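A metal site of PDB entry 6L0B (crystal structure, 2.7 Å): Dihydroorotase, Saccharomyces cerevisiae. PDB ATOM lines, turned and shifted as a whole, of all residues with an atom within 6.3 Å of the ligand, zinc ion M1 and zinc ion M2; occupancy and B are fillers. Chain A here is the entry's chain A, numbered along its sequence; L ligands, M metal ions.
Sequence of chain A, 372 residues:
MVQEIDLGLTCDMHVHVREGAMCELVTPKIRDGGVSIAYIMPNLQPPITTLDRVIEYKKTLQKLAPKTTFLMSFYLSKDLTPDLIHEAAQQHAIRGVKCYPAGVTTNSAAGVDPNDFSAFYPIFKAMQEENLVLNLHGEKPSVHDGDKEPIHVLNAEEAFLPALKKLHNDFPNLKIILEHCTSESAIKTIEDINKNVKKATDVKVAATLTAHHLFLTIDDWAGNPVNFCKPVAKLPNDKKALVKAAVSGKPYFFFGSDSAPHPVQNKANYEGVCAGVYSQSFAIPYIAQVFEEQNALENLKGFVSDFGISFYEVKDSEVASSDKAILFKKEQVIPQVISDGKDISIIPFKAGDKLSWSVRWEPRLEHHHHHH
A fluorine (F1) of the ligand sits close to the side-chain hydroxyl (OG1) of Thr 106, 2.7 Å away.
A ring nitrogen (NE2) of His 262 sits close to a fluorine (F1) of the ligand (2.6 Å).
A fluorine (F1) of the ligand sits close to the backbone carbonyl oxygen of Ala 275, at 2.9 Å.
Lys 230 touches the ligand (O to O1, 3.9 Å).
Ala 260 touches the ligand (CB to C3, 3.5 Å).
Gly 276 touches the ligand (CA to C4, 3.7 Å).
Hydrophobic or aromatic side chains within 4 Å of the ligand: His 16, His 137, Ala 260, His 262 and Ala 275.
Within 4 Å of the ligand: His 16, Arg 18, Asn 43, KCX 98, Thr 105, Thr 106, His 137, Lys 230, Asp 258, Ala 260, His 262, Ala 275 and Gly 276.
The nearest printed residue that does not touch the ligand is His 180 (4.1 Å).
O2 of the ligand sits at hydrogen-bond distance from ND2 of Asn 43 (2.8 Å).
A ring nitrogen (ND1) of His 16 is in hydrogen-bond range of an oxygen (O2) of the ligand, 3.2 Å away.
The guanidinium group (NH1) of Arg 18 lies within hydrogen-bond range of an oxygen (O2) of the ligand, at 2.7 Å.
The side-chain hydroxyl (OG1) of Thr 105 sits at hydrogen-bond distance from a nitrogen (N1) of the ligand, 2.9 Å away.
Along chain A the residues within 4 Å of zinc ion M1 span positions 98 to 180.
Zinc ion M2 is bound by a ring nitrogen (NE2) of His 16, a ring nitrogen (NE2) of His 14, OQ1 of KCX 98 and the side-chain carboxylate of Asp 258.
Zinc ion M1 is bound by a ring nitrogen (ND1) of His 137 (2.1 Å), OQ2 of KCX 98 (2.1 Å), a ring nitrogen (NE2) of His 180 (2.4 Å) and an oxygen (O1) of the ligand (2.4 Å).
N of Ala 260 sits at hydrogen-bond distance from O of Val 277 (2.9 Å).
A ring nitrogen (ND1) of His 16 sits at hydrogen-bond distance from the side-chain amide oxygen of Asn 43 (3.0 Å).
ND2 of Asn 107 is in hydrogen-bond range of O of Asn 43.
The backbone carbonyl oxygen (O) of Ala 275 lies within hydrogen-bond range of a ring nitrogen (NE2) of His 262 (2.5 Å).
A ring nitrogen (NE2) of His 262 sits at hydrogen-bond distance from the guanidinium group of Arg 18.
NZ of KCX 98 sits at hydrogen-bond distance from SD of Met 41 (3.6 Å).
The guanidinium group of Arg 18 sits at hydrogen-bond distance from the backbone carbonyl oxygen of Pro 261, 2.7 Å away.
OH of Tyr 100 lies within hydrogen-bond range of NZ of KCX 98 (3.4 Å).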
ATOM      1  N   HIS A  14      14.362  -2.752  27.173  1.00  0.00           N
ATOM      2  CA  HIS A  14      13.026  -2.321  26.763  1.00  0.00           C
ATOM      3  C   HIS A  14      12.333  -1.748  28.000  1.00  0.00           C
ATOM      4  O   HIS A  14      11.650  -2.471  28.725  1.00  0.00           O
ATOM      5  CB  HIS A  14      12.227  -3.453  26.162  1.00  0.00           C
ATOM      6  CG  HIS A  14      11.064  -3.010  25.341  1.00  0.00           C
ATOM      7  ND1 HIS A  14      10.889  -3.393  24.033  1.00  0.00           N
ATOM      8  CD2 HIS A  14      10.005  -2.208  25.636  1.00  0.00           C
ATOM      9  CE1 HIS A  14       9.772  -2.863  23.555  1.00  0.00           C
ATOM     10  NE2 HIS A  14       9.223  -2.148  24.513  1.00  0.00           N
ATOM     11  N   VAL A  15      12.477  -0.458  28.213  1.00  0.00           N
ATOM     12  CA  VAL A  15      11.995   0.191  29.419  1.00  0.00           C
ATOM     13  C   VAL A  15      11.126   1.367  29.017  1.00  0.00           C
ATOM     14  O   VAL A  15      11.420   2.070  28.046  1.00  0.00           O
ATOM     15  CB  VAL A  15      13.153   0.641  30.320  1.00  0.00           C
ATOM     16  CG1 VAL A  15      12.623   1.376  31.537  1.00  0.00           C
ATOM     17  CG2 VAL A  15      14.034  -0.531  30.741  1.00  0.00           C
ATOM     18  N   HIS A  16       9.998   1.549  29.719  1.00  0.00           N
ATOM     19  CA  HIS A  16       9.209   2.769  29.666  1.00  0.00           C
ATOM     20  C   HIS A  16       9.120   3.385  31.059  1.00  0.00           C
ATOM     21  O   HIS A  16       8.770   2.681  32.007  1.00  0.00           O
ATOM     22  CB  HIS A  16       7.793   2.510  29.100  1.00  0.00           C
ATOM     23  CG  HIS A  16       7.772   1.818  27.765  1.00  0.00           C
ATOM     24  ND1 HIS A  16       7.249   2.405  26.633  1.00  0.00           N
ATOM     25  CD2 HIS A  16       8.186   0.582  27.390  1.00  0.00           C
ATOM     26  CE1 HIS A  16       7.378   1.584  25.610  1.00  0.00           C
ATOM     27  NE2 HIS A  16       7.946   0.469  26.041  1.00  0.00           N
ATOM     28  N   ARG A  18       7.896   6.982  31.360  1.00  0.00           N
ATOM     29  CA  ARG A  18       6.931   8.094  31.283  1.00  0.00           C
ATOM     30  C   ARG A  18       7.626   9.396  31.686  1.00  0.00           C
ATOM     31  O   ARG A  18       8.829   9.575  31.484  1.00  0.00           O
ATOM     32  CB  ARG A  18       5.683   7.775  32.110  1.00  0.00           C
ATOM     33  CG  ARG A  18       5.156   6.335  32.030  1.00  0.00           C
ATOM     34  CD  ARG A  18       4.550   5.960  30.661  1.00  0.00           C
ATOM     35  NE  ARG A  18       3.869   4.653  30.649  1.00  0.00           N
ATOM     36  CZ  ARG A  18       3.765   3.809  29.608  1.00  0.00           C
ATOM     37  NH1 ARG A  18       4.310   4.056  28.405  1.00  0.00           N
ATOM     38  NH2 ARG A  18       3.123   2.661  29.786  1.00  0.00           N
ATOM     39  N   MET A  41      12.597   4.034  26.184  1.00  0.00           N
ATOM     40  CA  MET A  41      11.746   4.075  25.001  1.00  0.00           C
ATOM     41  C   MET A  41      11.144   5.466  24.772  1.00  0.00           C
ATOM     42  O   MET A  41      11.057   6.277  25.705  1.00  0.00           O
ATOM     43  CB  MET A  41      10.637   3.026  25.111  1.00  0.00           C
ATOM     44  CG  MET A  41      11.117   1.602  24.783  1.00  0.00           C
ATOM     45  SD  MET A  41      11.880   1.386  23.150  1.00  0.00           S
ATOM     46  CE  MET A  41      12.349  -0.364  23.236  1.00  0.00           C
ATOM     47  N   ASN A  43       8.049   6.696  23.443  1.00  0.00           N
ATOM     48  CA  ASN A  43       6.628   6.935  23.178  1.00  0.00           C
ATOM     49  C   ASN A  43       5.994   7.775  24.284  1.00  0.00           C
ATOM     50  O   ASN A  43       5.066   7.357  24.994  1.00  0.00           O
ATOM     51  CB  ASN A  43       5.918   5.597  23.001  1.00  0.00           C
ATOM     52  CG  ASN A  43       5.893   4.789  24.278  1.00  0.00           C
ATOM     53  OD1 ASN A  43       6.744   5.004  25.154  1.00  0.00           O
ATOM     54  ND2 ASN A  43       4.912   3.891  24.408  1.00  0.00           N
ATOM     55  N   KCX A  98      13.096   3.511  17.769  1.00  0.00           N
ATOM     56  CA  KCX A  98      12.027   2.549  18.015  1.00  0.00           C
ATOM     57  CB  KCX A  98      11.542   2.585  19.476  1.00  0.00           C
ATOM     58  CG  KCX A  98      10.273   1.759  19.749  1.00  0.00           C
ATOM     59  CD  KCX A  98      10.574   0.271  19.517  1.00  0.00           C
ATOM     60  CE  KCX A  98       9.480  -0.627  20.032  1.00  0.00           C
ATOM     61  NZ  KCX A  98       9.084   0.018  21.291  1.00  0.00           N
ATOM     62  C   KCX A  98      10.862   2.854  17.116  1.00  0.00           C
ATOM     63  O   KCX A  98      10.352   3.973  17.077  1.00  0.00           O
ATOM     64  CX  KCX A  98       8.218  -0.507  22.146  1.00  0.00           C
ATOM     65  OQ1 KCX A  98       7.947   0.117  23.175  1.00  0.00           O
ATOM     66  OQ2 KCX A  98       7.706  -1.615  21.942  1.00  0.00           O
ATOM     67  N   TYR A 100       7.008   2.215  16.010  1.00  0.00           N
ATOM     68  CA  TYR A 100       5.665   1.798  16.419  1.00  0.00           C
ATOM     69  C   TYR A 100       4.762   1.762  15.197  1.00  0.00           C
ATOM     70  O   TYR A 100       4.502   2.831  14.606  1.00  0.00           O
ATOM     71  CB  TYR A 100       5.066   2.748  17.473  1.00  0.00           C
ATOM     72  CG  TYR A 100       5.751   2.760  18.830  1.00  0.00           C
ATOM     73  CD1 TYR A 100       5.430   1.840  19.832  1.00  0.00           C
ATOM     74  CD2 TYR A 100       6.732   3.707  19.106  1.00  0.00           C
ATOM     75  CE1 TYR A 100       6.066   1.862  21.074  1.00  0.00           C
ATOM     76  CE2 TYR A 100       7.374   3.736  20.337  1.00  0.00           C
ATOM     77  CZ  TYR A 100       7.042   2.833  21.317  1.00  0.00           C
ATOM     78  OH  TYR A 100       7.715   2.905  22.511  1.00  0.00           O
ATOM     79  N   THR A 105      -0.486   0.118  19.777  1.00  0.00           N
ATOM     80  CA  THR A 105      -0.180   0.120  21.204  1.00  0.00           C
ATOM     81  C   THR A 105      -0.218   1.552  21.727  1.00  0.00           C
ATOM     82  O   THR A 105      -0.575   2.486  21.001  1.00  0.00           O
ATOM     83  CB  THR A 105       1.195  -0.531  21.438  1.00  0.00           C
ATOM     84  OG1 THR A 105       1.476  -0.564  22.833  1.00  0.00           O
ATOM     85  CG2 THR A 105       2.275   0.276  20.720  1.00  0.00           C
ATOM     86  N   THR A 106       0.244   1.745  22.967  1.00  0.00           N
ATOM     87  CA  THR A 106       0.180   3.045  23.648  1.00  0.00           C
ATOM     88  C   THR A 106       1.008   4.086  22.915  1.00  0.00           C
ATOM     89  O   THR A 106       2.175   3.848  22.606  1.00  0.00           O
ATOM     90  CB  THR A 106       0.730   2.933  25.070  1.00  0.00           C
ATOM     91  OG1 THR A 106      -0.062   2.045  25.862  1.00  0.00           O
ATOM     92  CG2 THR A 106       0.771   4.289  25.743  1.00  0.00           C
ATOM     93  N   ASN A 107       0.412   5.261  22.680  1.00  0.00           N
ATOM     94  CA  ASN A 107       1.116   6.383  22.068  1.00  0.00           C
ATOM     95  C   ASN A 107       1.776   5.969  20.750  1.00  0.00           C
ATOM     96  O   ASN A 107       2.959   6.208  20.535  1.00  0.00           O
ATOM     97  CB  ASN A 107       2.143   6.995  23.032  1.00  0.00           C
ATOM     98  CG  ASN A 107       1.484   7.735  24.193  1.00  0.00           C
ATOM     99  OD1 ASN A 107       0.264   7.937  24.203  1.00  0.00           O
ATOM    100  ND2 ASN A 107       2.294   8.166  25.173  1.00  0.00           N
ATOM    101  N   HIS A 137       8.569  -2.840  17.139  1.00  0.00           N
ATOM    102  CA  HIS A 137       7.332  -3.423  17.662  1.00  0.00           C
ATOM    103  C   HIS A 137       6.638  -4.110  16.500  1.00  0.00           C
ATOM    104  O   HIS A 137       5.808  -3.520  15.825  1.00  0.00           O
ATOM    105  CB  HIS A 137       6.421  -2.379  18.290  1.00  0.00           C
ATOM    106  CG  HIS A 137       5.168  -2.955  18.897  1.00  0.00           C
ATOM    107  ND1 HIS A 137       4.866  -2.829  20.235  1.00  0.00           N
ATOM    108  CD2 HIS A 137       4.137  -3.649  18.342  1.00  0.00           C
ATOM    109  CE1 HIS A 137       3.710  -3.409  20.485  1.00  0.00           C
ATOM    110  NE2 HIS A 137       3.244  -3.908  19.347  1.00  0.00           N
ATOM    111  N   GLU A 179      11.357  -6.677  19.038  1.00  0.00           N
ATOM    112  CA  GLU A 179      11.043  -6.486  20.449  1.00  0.00           C
ATOM    113  C   GLU A 179       9.930  -7.401  20.921  1.00  0.00           C
ATOM    114  O   GLU A 179       8.990  -7.710  20.167  1.00  0.00           O
ATOM    115  CB  GLU A 179      10.620  -5.032  20.734  1.00  0.00           C
ATOM    116  CG  GLU A 179      11.696  -4.022  20.469  1.00  0.00           C
ATOM    117  CD  GLU A 179      12.750  -3.990  21.557  1.00  0.00           C
ATOM    118  OE1 GLU A 179      12.465  -4.371  22.710  1.00  0.00           O
ATOM    119  OE2 GLU A 179      13.875  -3.564  21.240  1.00  0.00           O
ATOM    120  N   HIS A 180       9.990  -7.740  22.215  1.00  0.00           N
ATOM    121  CA  HIS A 180       9.030  -8.584  22.930  1.00  0.00           C
ATOM    122  C   HIS A 180       8.376  -9.655  22.058  1.00  0.00           C
ATOM    123  O   HIS A 180       7.179  -9.557  21.748  1.00  0.00           O
ATOM    124  CB  HIS A 180       7.947  -7.715  23.612  1.00  0.00           C
ATOM    125  CG  HIS A 180       7.426  -6.568  22.784  1.00  0.00           C
ATOM    126  ND1 HIS A 180       7.164  -6.680  21.433  1.00  0.00           N
ATOM    127  CD2 HIS A 180       7.054  -5.316  23.145  1.00  0.00           C
ATOM    128  CE1 HIS A 180       6.706  -5.522  20.988  1.00  0.00           C
ATOM    129  NE2 HIS A 180       6.627  -4.685  22.003  1.00  0.00           N
ATOM    130  N   CYS A 229      -1.563  -6.535  27.425  1.00  0.00           N
ATOM    131  CA  CYS A 229      -0.433  -5.797  26.885  1.00  0.00           C
ATOM    132  C   CYS A 229      -0.373  -6.046  25.380  1.00  0.00           C
ATOM    133  O   CYS A 229      -1.100  -6.884  24.840  1.00  0.00           O
ATOM    134  CB  CYS A 229       0.867  -6.188  27.587  1.00  0.00           C
ATOM    135  SG  CYS A 229       1.511  -7.804  27.105  1.00  0.00           S
ATOM    136  N   LYS A 230       0.518  -5.315  24.696  1.00  0.00           N
ATOM    137  CA  LYS A 230       0.729  -5.556  23.269  1.00  0.00           C
ATOM    138  C   LYS A 230       2.200  -5.903  23.051  1.00  0.00           C
ATOM    139  O   LYS A 230       3.061  -5.277  23.685  1.00  0.00           O
ATOM    140  CB  LYS A 230       0.333  -4.338  22.418  1.00  0.00           C
ATOM    141  CG  LYS A 230      -1.146  -3.948  22.490  1.00  0.00           C
ATOM    142  CD  LYS A 230      -2.043  -5.096  22.095  1.00  0.00           C
ATOM    143  CE  LYS A 230      -1.990  -5.392  20.608  1.00  0.00           C
ATOM    144  NZ  LYS A 230      -2.858  -4.466  19.822  1.00  0.00           N
ATOM    145  N   PRO A 231       2.529  -6.967  22.288  1.00  0.00           N
ATOM    146  CA  PRO A 231       1.564  -7.913  21.711  1.00  0.00           C
ATOM    147  C   PRO A 231       0.945  -8.768  22.815  1.00  0.00           C
ATOM    148  O   PRO A 231       1.586  -9.003  23.843  1.00  0.00           O
ATOM    149  CB  PRO A 231       2.403  -8.771  20.770  1.00  0.00           C
ATOM    150  CG  PRO A 231       3.677  -8.022  20.578  1.00  0.00           C
ATOM    151  CD  PRO A 231       3.897  -7.216  21.818  1.00  0.00           C
ATOM    152  N   ASP A 258       9.898  -4.474  28.755  1.00  0.00           N
ATOM    153  CA  ASP A 258       8.732  -3.666  28.386  1.00  0.00           C
ATOM    154  C   ASP A 258       7.842  -3.424  29.602  1.00  0.00           C
ATOM    155  O   ASP A 258       6.622  -3.530  29.550  1.00  0.00           O
ATOM    156  CB  ASP A 258       7.937  -4.312  27.249  1.00  0.00           C
ATOM    157  CG  ASP A 258       6.775  -3.438  26.748  1.00  0.00           C
ATOM    158  OD1 ASP A 258       6.793  -2.196  26.944  1.00  0.00           O
ATOM    159  OD2 ASP A 258       5.852  -3.986  26.131  1.00  0.00           O
ATOM    160  N   SER A 259       8.470  -3.110  30.724  1.00  0.00           N
ATOM    161  CA  SER A 259       7.662  -2.648  31.834  1.00  0.00           C
ATOM    162  C   SER A 259       7.016  -1.347  31.396  1.00  0.00           C
ATOM    163  O   SER A 259       7.714  -0.384  31.067  1.00  0.00           O
ATOM    164  CB  SER A 259       8.530  -2.514  33.084  1.00  0.00           C
ATOM    165  OG  SER A 259       7.776  -2.063  34.204  1.00  0.00           O
ATOM    166  N   ALA A 260       5.676  -1.331  31.315  1.00  0.00           N
ATOM    167  CA  ALA A 260       4.895  -0.190  30.808  1.00  0.00           C
ATOM    168  C   ALA A 260       3.885   0.251  31.869  1.00  0.00           C
ATOM    169  O   ALA A 260       2.753  -0.239  31.910  1.00  0.00           O
ATOM    170  CB  ALA A 260       4.190  -0.557  29.507  1.00  0.00           C
ATOM    171  N   PRO A 261       4.262   1.199  32.731  1.00  0.00           N
ATOM    172  CA  PRO A 261       3.373   1.601  33.828  1.00  0.00           C
ATOM    173  C   PRO A 261       2.217   2.470  33.356  1.00  0.00           C
ATOM    174  O   PRO A 261       2.362   3.246  32.411  1.00  0.00           O
ATOM    175  CB  PRO A 261       4.318   2.340  34.798  1.00  0.00           C
ATOM    176  CG  PRO A 261       5.462   2.809  33.933  1.00  0.00           C
ATOM    177  CD  PRO A 261       5.595   1.835  32.804  1.00  0.00           C
ATOM    178  N   HIS A 262       1.044   2.268  33.963  1.00  0.00           N
ATOM    179  CA  HIS A 262      -0.180   3.090  33.807  1.00  0.00           C
ATOM    180  C   HIS A 262      -0.844   3.177  35.172  1.00  0.00           C
ATOM    181  O   HIS A 262      -0.828   2.193  35.929  1.00  0.00           O
ATOM    182  CB  HIS A 262      -1.203   2.523  32.811  1.00  0.00           C
ATOM    183  CG  HIS A 262      -0.630   2.171  31.475  1.00  0.00           C
ATOM    184  ND1 HIS A 262      -0.865   2.939  30.347  1.00  0.00           N
ATOM    185  CD2 HIS A 262       0.098   1.106  31.062  1.00  0.00           C
ATOM    186  CE1 HIS A 262      -0.259   2.389  29.313  1.00  0.00           C
ATOM    187  NE2 HIS A 262       0.333   1.279  29.723  1.00  0.00           N
ATOM    188  N   CYS A 274      -5.805   0.558  28.745  1.00  0.00           N
ATOM    189  CA  CYS A 274      -4.437   0.837  28.311  1.00  0.00           C
ATOM    190  C   CYS A 274      -3.609  -0.438  28.305  1.00  0.00           C
ATOM    191  O   CYS A 274      -3.591  -1.194  29.286  1.00  0.00           O
ATOM    192  CB  CYS A 274      -3.797   1.866  29.232  1.00  0.00           C
ATOM    193  SG  CYS A 274      -4.588   3.456  29.237  1.00  0.00           S
ATOM    194  N   ALA A 275      -2.904  -0.688  27.205  1.00  0.00           N
ATOM    195  CA  ALA A 275      -1.991  -1.817  27.134  1.00  0.00           C
ATOM    196  C   ALA A 275      -0.754  -1.564  27.986  1.00  0.00           C
ATOM    197  O   ALA A 275      -0.240  -0.444  28.046  1.00  0.00           O
ATOM    198  CB  ALA A 275      -1.589  -2.071  25.683  1.00  0.00           C
ATOM    199  N   GLY A 276      -0.252  -2.622  28.638  1.00  0.00           N
ATOM    200  CA  GLY A 276       0.987  -2.508  29.404  1.00  0.00           C
ATOM    201  C   GLY A 276       1.040  -3.204  30.750  1.00  0.00           C
ATOM    202  O   GLY A 276       0.158  -3.054  31.610  1.00  0.00           O
ATOM    203  N   VAL A 277       2.117  -3.947  30.967  1.00  0.00           N
ATOM    204  CA  VAL A 277       2.326  -4.636  32.228  1.00  0.00           C
ATOM    205  C   VAL A 277       3.507  -3.995  32.910  1.00  0.00           C
ATOM    206  O   VAL A 277       4.580  -3.850  32.302  1.00  0.00           O
ATOM    207  CB  VAL A 277       2.562  -6.139  32.008  1.00  0.00           C
ATOM    208  CG1 VAL A 277       2.980  -6.781  33.303  1.00  0.00           C
ATOM    209  CG2 VAL A 277       1.297  -6.799  31.470  1.00  0.00           C
HETATM  210  N1  LIG L   1       2.672  -1.472  25.342  1.00  0.00           N
HETATM  211  C1  LIG L   1       3.905  -1.001  24.662  1.00  0.00           C
HETATM  212  N2  LIG L   1       4.404   0.349  25.055  1.00  0.00           N
HETATM  213  C2  LIG L   1       3.700   1.144  26.068  1.00  0.00           C
HETATM  214  C3  LIG L   1       2.479   0.655  26.711  1.00  0.00           C
HETATM  215  C4  LIG L   1       1.999  -0.645  26.319  1.00  0.00           C
HETATM  216  O1  LIG L   1       4.459  -1.671  23.828  1.00  0.00           O
HETATM  217  O2  LIG L   1       4.058   2.210  26.438  1.00  0.00           O
HETATM  218  F1  LIG L   1       1.883   1.498  27.636  1.00  0.00           F
HETATM  219 ZN    ZN M   1       5.780  -2.493  22.052  1.00  0.00          ZN
HETATM  220 ZN    ZN M   2       7.252  -1.174  24.893  1.00  0.00          ZN
